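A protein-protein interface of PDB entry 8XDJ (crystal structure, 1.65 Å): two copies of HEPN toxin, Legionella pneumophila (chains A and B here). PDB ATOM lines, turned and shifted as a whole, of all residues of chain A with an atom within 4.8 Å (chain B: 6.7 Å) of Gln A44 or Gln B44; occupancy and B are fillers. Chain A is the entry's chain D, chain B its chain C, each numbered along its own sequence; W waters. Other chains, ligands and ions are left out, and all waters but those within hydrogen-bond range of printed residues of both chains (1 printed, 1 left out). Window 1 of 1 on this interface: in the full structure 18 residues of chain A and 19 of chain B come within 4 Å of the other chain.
OE2 of Glu A47 sits close to OE1 of Gln B44 (2.7 Å).
The side-chain amide nitrogen (NE2) of Gln B44 lies within hydrogen-bond range of the backbone carbonyl oxygen (O) of Thr A101 (2.9 Å).
NE2 of Gln B44 lies within hydrogen-bond range of OG1 of Thr A104.
OE2 of Glu B47 lies close to OE1 of Gln A44.
The side-chain amide nitrogen (NE2) of Gln A44 lies within hydrogen-bond range of the backbone carbonyl oxygen (O) of Thr B101.
The side-chain hydroxyl (OG1) of Thr B104 lies within hydrogen-bond range of the side-chain amide nitrogen (NE2) of Gln A44 (3.0 Å).
OE1 of Gln B40 lies within hydrogen-bond range of OG1 of Thr B104 (2.8 Å).
The side-chain amide oxygen (OE1) of Gln B44 lies close to the side-chain carboxylate (OE2) of Glu B47, 3.4 Å away.
The side-chain hydroxyl of Thr B104 sits at hydrogen-bond distance from the backbone carbonyl oxygen of Thr B101.
O of Thr A104 is in hydrogen-bond range of NE2 of Gln A40, at 2.7 Å.
OE1 of Glu A47 sits at hydrogen-bond distance from OG1 of Thr A101, 3.2 Å away.
O of Thr A101 is in hydrogen-bond range of OG1 of Thr A104 (3.2 Å).
C of Gln A40 touches CA of Gly B41, 3.7 Å away.
OE1 of Gln A40 touches CG of Gln B44 (3.3 Å).
Gln A40 touches Phe B48 (OE1 to CE2, 3.5 Å).
CA of Gly A41 touches C of Gln B40, at 3.7 Å.
CA of Gly A41 touches N of Gly B41 (3.3 Å).
Gln B40 touches Gln A44 (OE1 to CG, 3.4 Å).
OE1 of Gln A44 touches OE1 of Gln B44, at 3.7 Å.
Phe A48 touches Ser B102 (CB to O, 3.5 Å).
Phe A48 touches Thr B104.
Phe A48 touches Tyr B105 (CE1 to CB, 3.6 Å).
Of the printed residues of chain B, Gln A44 touches Gln B40 (3.4 Å), Gln B44 (3.7 Å), Glu B47 (2.7 Å), Thr B101 (2.9 Å) and Thr B104 (3.0 Å).
Gln B44 touches just these residues of chain A: Gln A40 (3.3 Å), Gln A44 (3.7 Å), Glu A47 (2.7 Å), Thr A101 (2.9 Å) and Thr A104 (2.9 Å).
Of the printed residues of chain A, Phe B48 touches Gln A40 (3.5 Å) and Thr A104 (3.3 Å).
Of the printed residues of chain A, Thr B104 touches Gln A44 (3.0 Å) and Phe A48 (3.4 Å).
Of the printed residues of chain B, Thr A101 touches Gln B44 (2.9 Å).
Of the printed residues of chain B, Thr A104 touches Gln B44 and Phe B48.
Of the printed residues of chain A, Tyr B105 touches Phe A48.
Ala B45 touches none of the printed residues of chain A.
The nearest residue of chain A that does not touch Gln B44 is Ile A43 (4.2 Å).
Of the 11 printed residues of chain A, 7 touch a printed residue of chain B.
Hydrophobic or aromatic side chains of chain A that line the printed part of chain B: Phe A48.
Among the printed residues, 19 pairs touch across the chains.
Gln A40 touches Gln B44, and with the chains exchanged Gln A44 touches Gln B40.
Gln A40 touches Phe B48, and with the chains exchanged Phe A48 touches Gln B40.
Gln A44 touches Thr B104, and with the chains exchanged Thr A104 touches Gln B44.
Glu A47 touches its own counterpart, Glu B47.
Positions printed for both chains: 40, 41, 42, 43, 44, 45, 46, 47, 48, 101 and 104.
Water W1 lies within hydrogen-bond range of O of Ser B102 and O of Phe A48.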
ATOM      1  N   GLN A  40     -21.518 -32.229   0.677  1.00  0.00           N
ATOM      2  CA  GLN A  40     -20.396 -31.461   0.155  1.00  0.00           C
ATOM      3  C   GLN A  40     -19.183 -31.587   1.055  1.00  0.00           C
ATOM      4  O   GLN A  40     -18.052 -31.557   0.564  1.00  0.00           O
ATOM      5  CB  GLN A  40     -20.765 -29.973   0.017  1.00  0.00           C
ATOM      6  CG  GLN A  40     -22.020 -29.757  -0.860  1.00  0.00           C
ATOM      7  CD  GLN A  40     -21.781 -30.083  -2.334  1.00  0.00           C
ATOM      8  OE1 GLN A  40     -20.663 -30.022  -2.806  1.00  0.00           O
ATOM      9  NE2 GLN A  40     -22.849 -30.423  -3.065  1.00  0.00           N
ATOM     10  N   GLY A  41     -19.403 -31.726   2.369  1.00  0.00           N
ATOM     11  CA  GLY A  41     -18.271 -31.916   3.286  1.00  0.00           C
ATOM     12  C   GLY A  41     -17.570 -33.247   3.090  1.00  0.00           C
ATOM     13  O   GLY A  41     -16.336 -33.340   3.214  1.00  0.00           O
ATOM     14  N   LEU A  42     -18.348 -34.302   2.819  1.00  0.00           N
ATOM     15  CA  LEU A  42     -17.775 -35.610   2.505  1.00  0.00           C
ATOM     16  C   LEU A  42     -16.938 -35.531   1.242  1.00  0.00           C
ATOM     17  O   LEU A  42     -15.844 -36.106   1.168  1.00  0.00           O
ATOM     18  CB  LEU A  42     -18.891 -36.664   2.364  1.00  0.00           C
ATOM     19  CG  LEU A  42     -18.440 -38.069   1.941  1.00  0.00           C
ATOM     20  CD1 LEU A  42     -17.612 -38.665   3.039  1.00  0.00           C
ATOM     21  CD2 LEU A  42     -19.677 -38.900   1.713  1.00  0.00           C
ATOM     22  N   ILE A  43     -17.409 -34.771   0.253  1.00  0.00           N
ATOM     23  CA  ILE A  43     -16.623 -34.596  -0.956  1.00  0.00           C
ATOM     24  C   ILE A  43     -15.328 -33.847  -0.654  1.00  0.00           C
ATOM     25  O   ILE A  43     -14.257 -34.233  -1.136  1.00  0.00           O
ATOM     26  CB  ILE A  43     -17.477 -33.889  -2.019  1.00  0.00           C
ATOM     27  CG1 ILE A  43     -18.609 -34.840  -2.442  1.00  0.00           C
ATOM     28  CG2 ILE A  43     -16.575 -33.409  -3.220  1.00  0.00           C
ATOM     29  CD1 ILE A  43     -19.724 -34.086  -3.299  1.00  0.00           C
ATOM     30  N   GLN A  44     -15.394 -32.772   0.141  1.00  0.00           N
ATOM     31  CA  GLN A  44     -14.166 -32.052   0.504  1.00  0.00           C
ATOM     32  C   GLN A  44     -13.188 -32.958   1.273  1.00  0.00           C
ATOM     33  O   GLN A  44     -11.970 -32.883   1.054  1.00  0.00           O
ATOM     34  CB  GLN A  44     -14.514 -30.779   1.295  1.00  0.00           C
ATOM     35  CG  GLN A  44     -13.329 -29.964   1.880  1.00  0.00           C
ATOM     36  CD  GLN A  44     -12.336 -29.471   0.844  1.00  0.00           C
ATOM     37  OE1 GLN A  44     -12.610 -29.470  -0.345  1.00  0.00           O
ATOM     38  NE2 GLN A  44     -11.155 -29.090   1.300  1.00  0.00           N
ATOM     39  N   ALA A  45     -13.691 -33.807   2.177  1.00  0.00           N
ATOM     40  CA  ALA A  45     -12.807 -34.735   2.878  1.00  0.00           C
ATOM     41  C   ALA A  45     -12.208 -35.751   1.914  1.00  0.00           C
ATOM     42  O   ALA A  45     -11.027 -36.096   2.026  1.00  0.00           O
ATOM     43  CB  ALA A  45     -13.548 -35.465   4.024  1.00  0.00           C
ATOM     44  N   PHE A  46     -12.995 -36.238   0.959  1.00  0.00           N
ATOM     45  CA  PHE A  46     -12.392 -37.049  -0.108  1.00  0.00           C
ATOM     46  C   PHE A  46     -11.268 -36.284  -0.821  1.00  0.00           C
ATOM     47  O   PHE A  46     -10.190 -36.835  -1.093  1.00  0.00           O
ATOM     48  CB  PHE A  46     -13.469 -37.480  -1.124  1.00  0.00           C
ATOM     49  CG  PHE A  46     -12.908 -37.847  -2.480  1.00  0.00           C
ATOM     50  CD1 PHE A  46     -12.184 -39.018  -2.643  1.00  0.00           C
ATOM     51  CD2 PHE A  46     -13.123 -37.032  -3.591  1.00  0.00           C
ATOM     52  CE1 PHE A  46     -11.646 -39.348  -3.910  1.00  0.00           C
ATOM     53  CE2 PHE A  46     -12.617 -37.371  -4.853  1.00  0.00           C
ATOM     54  CZ  PHE A  46     -11.851 -38.528  -4.998  1.00  0.00           C
ATOM     55  N   GLU A  47     -11.484 -35.002  -1.127  1.00  0.00           N
ATOM     56  CA  GLU A  47     -10.474 -34.248  -1.856  1.00  0.00           C
ATOM     57  C   GLU A  47      -9.180 -34.149  -1.063  1.00  0.00           C
ATOM     58  O   GLU A  47      -8.091 -34.336  -1.621  1.00  0.00           O
ATOM     59  CB  GLU A  47     -10.989 -32.843  -2.181  1.00  0.00           C
ATOM     60  CG  GLU A  47     -12.058 -32.843  -3.241  1.00  0.00           C
ATOM     61  CD  GLU A  47     -12.533 -31.406  -3.548  1.00  0.00           C
ATOM     62  OE1 GLU A  47     -11.844 -30.699  -4.307  1.00  0.00           O
ATOM     63  OE2 GLU A  47     -13.579 -30.974  -3.016  1.00  0.00           O
ATOM     64  N   PHE A  48      -9.260 -33.819   0.238  1.00  0.00           N
ATOM     65  CA  PHE A  48      -7.984 -33.669   0.929  1.00  0.00           C
ATOM     66  C   PHE A  48      -7.355 -35.027   1.265  1.00  0.00           C
ATOM     67  O   PHE A  48      -6.131 -35.106   1.335  1.00  0.00           O
ATOM     68  CB  PHE A  48      -8.047 -32.735   2.176  1.00  0.00           C
ATOM     69  CG  PHE A  48      -8.994 -33.121   3.345  1.00  0.00           C
ATOM     70  CD1 PHE A  48      -8.942 -34.350   3.992  1.00  0.00           C
ATOM     71  CD2 PHE A  48      -9.875 -32.149   3.858  1.00  0.00           C
ATOM     72  CE1 PHE A  48      -9.769 -34.634   5.079  1.00  0.00           C
ATOM     73  CE2 PHE A  48     -10.732 -32.427   4.942  1.00  0.00           C
ATOM     74  CZ  PHE A  48     -10.667 -33.679   5.565  1.00  0.00           C
ATOM     75  N   THR A 101     -15.165 -31.993  -9.092  1.00  0.00           N
ATOM     76  CA  THR A 101     -15.716 -31.410  -7.873  1.00  0.00           C
ATOM     77  C   THR A 101     -16.178 -29.975  -8.084  1.00  0.00           C
ATOM     78  O   THR A 101     -17.006 -29.502  -7.294  1.00  0.00           O
ATOM     79  CB  THR A 101     -14.752 -31.502  -6.688  1.00  0.00           C
ATOM     80  OG1 THR A 101     -13.577 -30.746  -6.947  1.00  0.00           O
ATOM     81  CG2 THR A 101     -14.408 -32.992  -6.395  1.00  0.00           C
ATOM     82  N   THR A 104     -20.194 -30.031  -8.268  1.00  0.00           N
ATOM     83  CA  THR A 104     -21.023 -30.670  -7.240  1.00  0.00           C
ATOM     84  C   THR A 104     -22.159 -29.795  -6.724  1.00  0.00           C
ATOM     85  O   THR A 104     -22.870 -30.220  -5.805  1.00  0.00           O
ATOM     86  CB  THR A 104     -20.192 -31.122  -6.027  1.00  0.00           C
ATOM     87  OG1 THR A 104     -19.565 -29.997  -5.380  1.00  0.00           O
ATOM     88  CG2 THR A 104     -19.107 -32.098  -6.460  1.00  0.00           C
ATOM     89  N   LEU B  22     -24.421 -21.849  -1.316  1.00  0.00           N
ATOM     90  CA  LEU B  22     -23.498 -21.239  -0.369  1.00  0.00           C
ATOM     91  C   LEU B  22     -24.239 -20.378   0.643  1.00  0.00           C
ATOM     92  O   LEU B  22     -23.939 -20.434   1.845  1.00  0.00           O
ATOM     93  CB  LEU B  22     -22.467 -20.387  -1.109  1.00  0.00           C
ATOM     94  CG  LEU B  22     -21.429 -19.700  -0.208  1.00  0.00           C
ATOM     95  CD1 LEU B  22     -20.712 -20.688   0.619  1.00  0.00           C
ATOM     96  CD2 LEU B  22     -20.419 -18.965  -1.065  1.00  0.00           C
ATOM     97  N   LYS B  39     -18.566 -27.660   8.134  1.00  0.00           N
ATOM     98  CA  LYS B  39     -17.545 -26.659   7.798  1.00  0.00           C
ATOM     99  C   LYS B  39     -16.841 -27.039   6.505  1.00  0.00           C
ATOM    100  O   LYS B  39     -16.589 -26.188   5.653  1.00  0.00           O
ATOM    101  CB  LYS B  39     -16.538 -26.551   8.956  1.00  0.00           C
ATOM    102  CG  LYS B  39     -17.073 -25.736  10.119  1.00  0.00           C
ATOM    103  CD  LYS B  39     -15.970 -25.271  11.055  1.00  0.00           C
ATOM    104  CE  LYS B  39     -16.552 -24.888  12.406  1.00  0.00           C
ATOM    105  NZ  LYS B  39     -15.486 -24.831  13.445  1.00  0.00           N
ATOM    106  N   GLN B  40     -16.519 -28.323   6.346  1.00  0.00           N
ATOM    107  CA  GLN B  40     -15.925 -28.772   5.107  1.00  0.00           C
ATOM    108  C   GLN B  40     -16.877 -28.580   3.956  1.00  0.00           C
ATOM    109  O   GLN B  40     -16.427 -28.288   2.846  1.00  0.00           O
ATOM    110  CB  GLN B  40     -15.531 -30.249   5.230  1.00  0.00           C
ATOM    111  CG  GLN B  40     -14.568 -30.527   6.361  1.00  0.00           C
ATOM    112  CD  GLN B  40     -13.226 -29.836   6.249  1.00  0.00           C
ATOM    113  OE1 GLN B  40     -12.774 -29.491   5.153  1.00  0.00           O
ATOM    114  NE2 GLN B  40     -12.535 -29.708   7.393  1.00  0.00           N
ATOM    115  N   GLY B  41     -18.184 -28.764   4.193  1.00  0.00           N
ATOM    116  CA  GLY B  41     -19.172 -28.519   3.149  1.00  0.00           C
ATOM    117  C   GLY B  41     -19.259 -27.061   2.727  1.00  0.00           C
ATOM    118  O   GLY B  41     -19.442 -26.773   1.554  1.00  0.00           O
ATOM    119  N   LEU B  42     -19.177 -26.134   3.686  1.00  0.00           N
ATOM    120  CA  LEU B  42     -19.151 -24.712   3.361  1.00  0.00           C
ATOM    121  C   LEU B  42     -17.933 -24.370   2.517  1.00  0.00           C
ATOM    122  O   LEU B  42     -18.022 -23.577   1.572  1.00  0.00           O
ATOM    123  CB  LEU B  42     -19.159 -23.897   4.650  1.00  0.00           C
ATOM    124  CG  LEU B  42     -19.193 -22.377   4.500  1.00  0.00           C
ATOM    125  CD1 LEU B  42     -20.458 -22.002   3.813  1.00  0.00           C
ATOM    126  CD2 LEU B  42     -19.171 -21.772   5.887  1.00  0.00           C
ATOM    127  N   ILE B  43     -16.784 -24.952   2.852  1.00  0.00           N
ATOM    128  CA  ILE B  43     -15.582 -24.724   2.064  1.00  0.00           C
ATOM    129  C   ILE B  43     -15.758 -25.251   0.644  1.00  0.00           C
ATOM    130  O   ILE B  43     -15.399 -24.574  -0.331  1.00  0.00           O
ATOM    131  CB  ILE B  43     -14.370 -25.355   2.768  1.00  0.00           C
ATOM    132  CG1 ILE B  43     -14.112 -24.616   4.083  1.00  0.00           C
ATOM    133  CG2 ILE B  43     -13.143 -25.374   1.819  1.00  0.00           C
ATOM    134  CD1 ILE B  43     -13.256 -25.381   5.071  1.00  0.00           C
ATOM    135  N   GLN B  44     -16.325 -26.453   0.497  1.00  0.00           N
ATOM    136  CA  GLN B  44     -16.605 -26.957  -0.856  1.00  0.00           C
ATOM    137  C   GLN B  44     -17.559 -26.029  -1.616  1.00  0.00           C
ATOM    138  O   GLN B  44     -17.334 -25.756  -2.801  1.00  0.00           O
ATOM    139  CB  GLN B  44     -17.168 -28.389  -0.799  1.00  0.00           C
ATOM    140  CG  GLN B  44     -17.632 -28.976  -2.135  1.00  0.00           C
ATOM    141  CD  GLN B  44     -16.514 -29.107  -3.154  1.00  0.00           C
ATOM    142  OE1 GLN B  44     -15.349 -28.936  -2.838  1.00  0.00           O
ATOM    143  NE2 GLN B  44     -16.880 -29.401  -4.399  1.00  0.00           N
ATOM    144  N   ALA B  45     -18.609 -25.509  -0.949  1.00  0.00           N
ATOM    145  CA  ALA B  45     -19.519 -24.576  -1.634  1.00  0.00           C
ATOM    146  C   ALA B  45     -18.796 -23.292  -2.035  1.00  0.00           C
ATOM    147  O   ALA B  45     -19.027 -22.749  -3.127  1.00  0.00           O
ATOM    148  CB  ALA B  45     -20.741 -24.258  -0.754  1.00  0.00           C
ATOM    149  N   PHE B  46     -17.851 -22.832  -1.206  1.00  0.00           N
ATOM    150  CA  PHE B  46     -17.016 -21.699  -1.606  1.00  0.00           C
ATOM    151  C   PHE B  46     -16.190 -22.040  -2.844  1.00  0.00           C
ATOM    152  O   PHE B  46     -16.089 -21.219  -3.757  1.00  0.00           O
ATOM    153  CB  PHE B  46     -16.111 -21.261  -0.438  1.00  0.00           C
ATOM    154  CG  PHE B  46     -14.871 -20.515  -0.871  1.00  0.00           C
ATOM    155  CD1 PHE B  46     -14.984 -19.215  -1.368  1.00  0.00           C
ATOM    156  CD2 PHE B  46     -13.621 -21.109  -0.796  1.00  0.00           C
ATOM    157  CE1 PHE B  46     -13.843 -18.533  -1.825  1.00  0.00           C
ATOM    158  CE2 PHE B  46     -12.468 -20.439  -1.220  1.00  0.00           C
ATOM    159  CZ  PHE B  46     -12.599 -19.137  -1.750  1.00  0.00           C
ATOM    160  N   GLU B  47     -15.616 -23.247  -2.910  1.00  0.00           N
ATOM    161  CA  GLU B  47     -14.810 -23.646  -4.063  1.00  0.00           C
ATOM    162  C   GLU B  47     -15.635 -23.610  -5.347  1.00  0.00           C
ATOM    163  O   GLU B  47     -15.173 -23.095  -6.369  1.00  0.00           O
ATOM    164  CB  GLU B  47     -14.248 -25.049  -3.850  1.00  0.00           C
ATOM    165  CG  GLU B  47     -13.090 -25.090  -2.834  1.00  0.00           C
ATOM    166  CD  GLU B  47     -12.644 -26.537  -2.582  1.00  0.00           C
ATOM    167  OE1 GLU B  47     -12.083 -27.165  -3.503  1.00  0.00           O
ATOM    168  OE2 GLU B  47     -12.848 -27.048  -1.467  1.00  0.00           O
ATOM    169  N   PHE B  48     -16.844 -24.179  -5.325  1.00  0.00           N
ATOM    170  CA  PHE B  48     -17.572 -24.221  -6.588  1.00  0.00           C
ATOM    171  C   PHE B  48     -18.205 -22.882  -6.929  1.00  0.00           C
ATOM    172  O   PHE B  48     -18.323 -22.566  -8.112  1.00  0.00           O
ATOM    173  CB  PHE B  48     -18.556 -25.415  -6.693  1.00  0.00           C
ATOM    174  CG  PHE B  48     -19.716 -25.490  -5.688  1.00  0.00           C
ATOM    175  CD1 PHE B  48     -20.631 -24.481  -5.505  1.00  0.00           C
ATOM    176  CD2 PHE B  48     -19.957 -26.709  -5.049  1.00  0.00           C
ATOM    177  CE1 PHE B  48     -21.717 -24.626  -4.624  1.00  0.00           C
ATOM    178  CE2 PHE B  48     -21.015 -26.867  -4.201  1.00  0.00           C
ATOM    179  CZ  PHE B  48     -21.903 -25.848  -3.975  1.00  0.00           C
ATOM    180  N   THR B  49     -18.533 -22.070  -5.927  1.00  0.00           N
ATOM    181  CA  THR B  49     -19.040 -20.737  -6.210  1.00  0.00           C
ATOM    182  C   THR B  49     -17.942 -19.837  -6.759  1.00  0.00           C
ATOM    183  O   THR B  49     -18.201 -19.037  -7.679  1.00  0.00           O
ATOM    184  CB  THR B  49     -19.641 -20.152  -4.939  1.00  0.00           C
ATOM    185  OG1 THR B  49     -20.718 -21.001  -4.547  1.00  0.00           O
ATOM    186  CG2 THR B  49     -20.255 -18.733  -5.191  1.00  0.00           C
ATOM    187  N   GLN B 100      -5.491 -23.057  -0.337  1.00  0.00           N
ATOM    188  CA  GLN B 100      -5.332 -23.701   0.954  1.00  0.00           C
ATOM    189  C   GLN B 100      -6.282 -24.857   1.180  1.00  0.00           C
ATOM    190  O   GLN B 100      -6.224 -25.444   2.252  1.00  0.00           O
ATOM    191  CB  GLN B 100      -5.537 -22.704   2.107  1.00  0.00           C
ATOM    192  CG  GLN B 100      -4.524 -21.570   2.153  1.00  0.00           C
ATOM    193  CD  GLN B 100      -3.139 -22.090   2.453  1.00  0.00           C
ATOM    194  OE1 GLN B 100      -2.774 -22.293   3.611  1.00  0.00           O
ATOM    195  NE2 GLN B 100      -2.357 -22.318   1.402  1.00  0.00           N
ATOM    196  N   THR B 101      -7.188 -25.176   0.241  1.00  0.00           N
ATOM    197  CA  THR B 101      -8.259 -26.058   0.678  1.00  0.00           C
ATOM    198  C   THR B 101      -7.780 -27.493   0.835  1.00  0.00           C
ATOM    199  O   THR B 101      -8.401 -28.249   1.578  1.00  0.00           O
ATOM    200  CB  THR B 101      -9.472 -26.025  -0.241  1.00  0.00           C
ATOM    201  OG1 THR B 101      -9.108 -26.537  -1.514  1.00  0.00           O
ATOM    202  CG2 THR B 101     -10.034 -24.597  -0.351  1.00  0.00           C
ATOM    203  N   SER B 102      -6.664 -27.871   0.210  1.00  0.00           N
ATOM    204  CA  SER B 102      -6.114 -29.197   0.529  1.00  0.00           C
ATOM    205  C   SER B 102      -5.639 -29.336   1.973  1.00  0.00           C
ATOM    206  O   SER B 102      -5.412 -30.470   2.436  1.00  0.00           O
ATOM    207  CB  SER B 102      -4.964 -29.510  -0.437  1.00  0.00           C
ATOM    208  OG  SER B 102      -3.776 -28.895   0.012  1.00  0.00           O
ATOM    209  N   HIS B 103      -5.519 -28.241   2.723  1.00  0.00           N
ATOM    210  CA  HIS B 103      -5.031 -28.289   4.093  1.00  0.00           C
ATOM    211  C   HIS B 103      -6.139 -28.204   5.130  1.00  0.00           C
ATOM    212  O   HIS B 103      -5.838 -28.095   6.323  1.00  0.00           O
ATOM    213  CB  HIS B 103      -4.003 -27.169   4.324  1.00  0.00           C
ATOM    214  CG  HIS B 103      -2.899 -27.156   3.317  1.00  0.00           C
ATOM    215  ND1 HIS B 103      -1.918 -28.127   3.281  1.00  0.00           N
ATOM    216  CD2 HIS B 103      -2.614 -26.295   2.310  1.00  0.00           C
ATOM    217  CE1 HIS B 103      -1.092 -27.879   2.277  1.00  0.00           C
ATOM    218  NE2 HIS B 103      -1.481 -26.761   1.685  1.00  0.00           N
ATOM    219  N   THR B 104      -7.414 -28.341   4.724  1.00  0.00           N
ATOM    220  CA  THR B 104      -8.509 -28.144   5.677  1.00  0.00           C
ATOM    221  C   THR B 104      -8.791 -29.350   6.572  1.00  0.00           C
ATOM    222  O   THR B 104      -9.721 -29.299   7.375  1.00  0.00           O
ATOM    223  CB  THR B 104      -9.811 -27.732   4.966  1.00  0.00           C
ATOM    224  OG1 THR B 104     -10.286 -28.780   4.127  1.00  0.00           O
ATOM    225  CG2 THR B 104      -9.616 -26.465   4.171  1.00  0.00           C
ATOM    226  N   TYR B 105      -7.983 -30.400   6.495  1.00  0.00           N
ATOM    227  CA  TYR B 105      -8.015 -31.418   7.520  1.00  0.00           C
ATOM    228  C   TYR B 105      -7.360 -30.939   8.819  1.00  0.00           C
ATOM    229  O   TYR B 105      -7.434 -31.639   9.824  1.00  0.00           O
ATOM    230  CB  TYR B 105      -7.355 -32.691   6.978  1.00  0.00           C
ATOM    231  CG  TYR B 105      -5.888 -32.548   6.691  1.00  0.00           C
ATOM    232  CD1 TYR B 105      -4.938 -32.812   7.689  1.00  0.00           C
ATOM    233  CD2 TYR B 105      -5.440 -32.144   5.446  1.00  0.00           C
ATOM    234  CE1 TYR B 105      -3.602 -32.686   7.434  1.00  0.00           C
ATOM    235  CE2 TYR B 105      -4.091 -32.005   5.188  1.00  0.00           C
ATOM    236  CZ  TYR B 105      -3.185 -32.302   6.212  1.00  0.00           C
ATOM    237  OH  TYR B 105      -1.869 -32.187   5.945  1.00  0.00           O
ATOM    238  N   ILE B 117     -15.031 -16.847   4.501  1.00  0.00           N
ATOM    239  CA  ILE B 117     -16.219 -17.068   3.667  1.00  0.00           C
ATOM    240  C   ILE B 117     -17.414 -16.312   4.229  1.00  0.00           C
ATOM    241  O   ILE B 117     -18.117 -15.574   3.516  1.00  0.00           O
ATOM    242  CB  ILE B 117     -16.521 -18.579   3.567  1.00  0.00           C
ATOM    243  CG1 ILE B 117     -15.441 -19.295   2.753  1.00  0.00           C
ATOM    244  CG2 ILE B 117     -17.897 -18.809   2.892  1.00  0.00           C
ATOM    245  CD1 ILE B 117     -15.552 -20.868   2.871  1.00  0.00           C
HETATM  246  O   HOH W   1      -4.526 -32.711   1.217  1.00  0.00           O
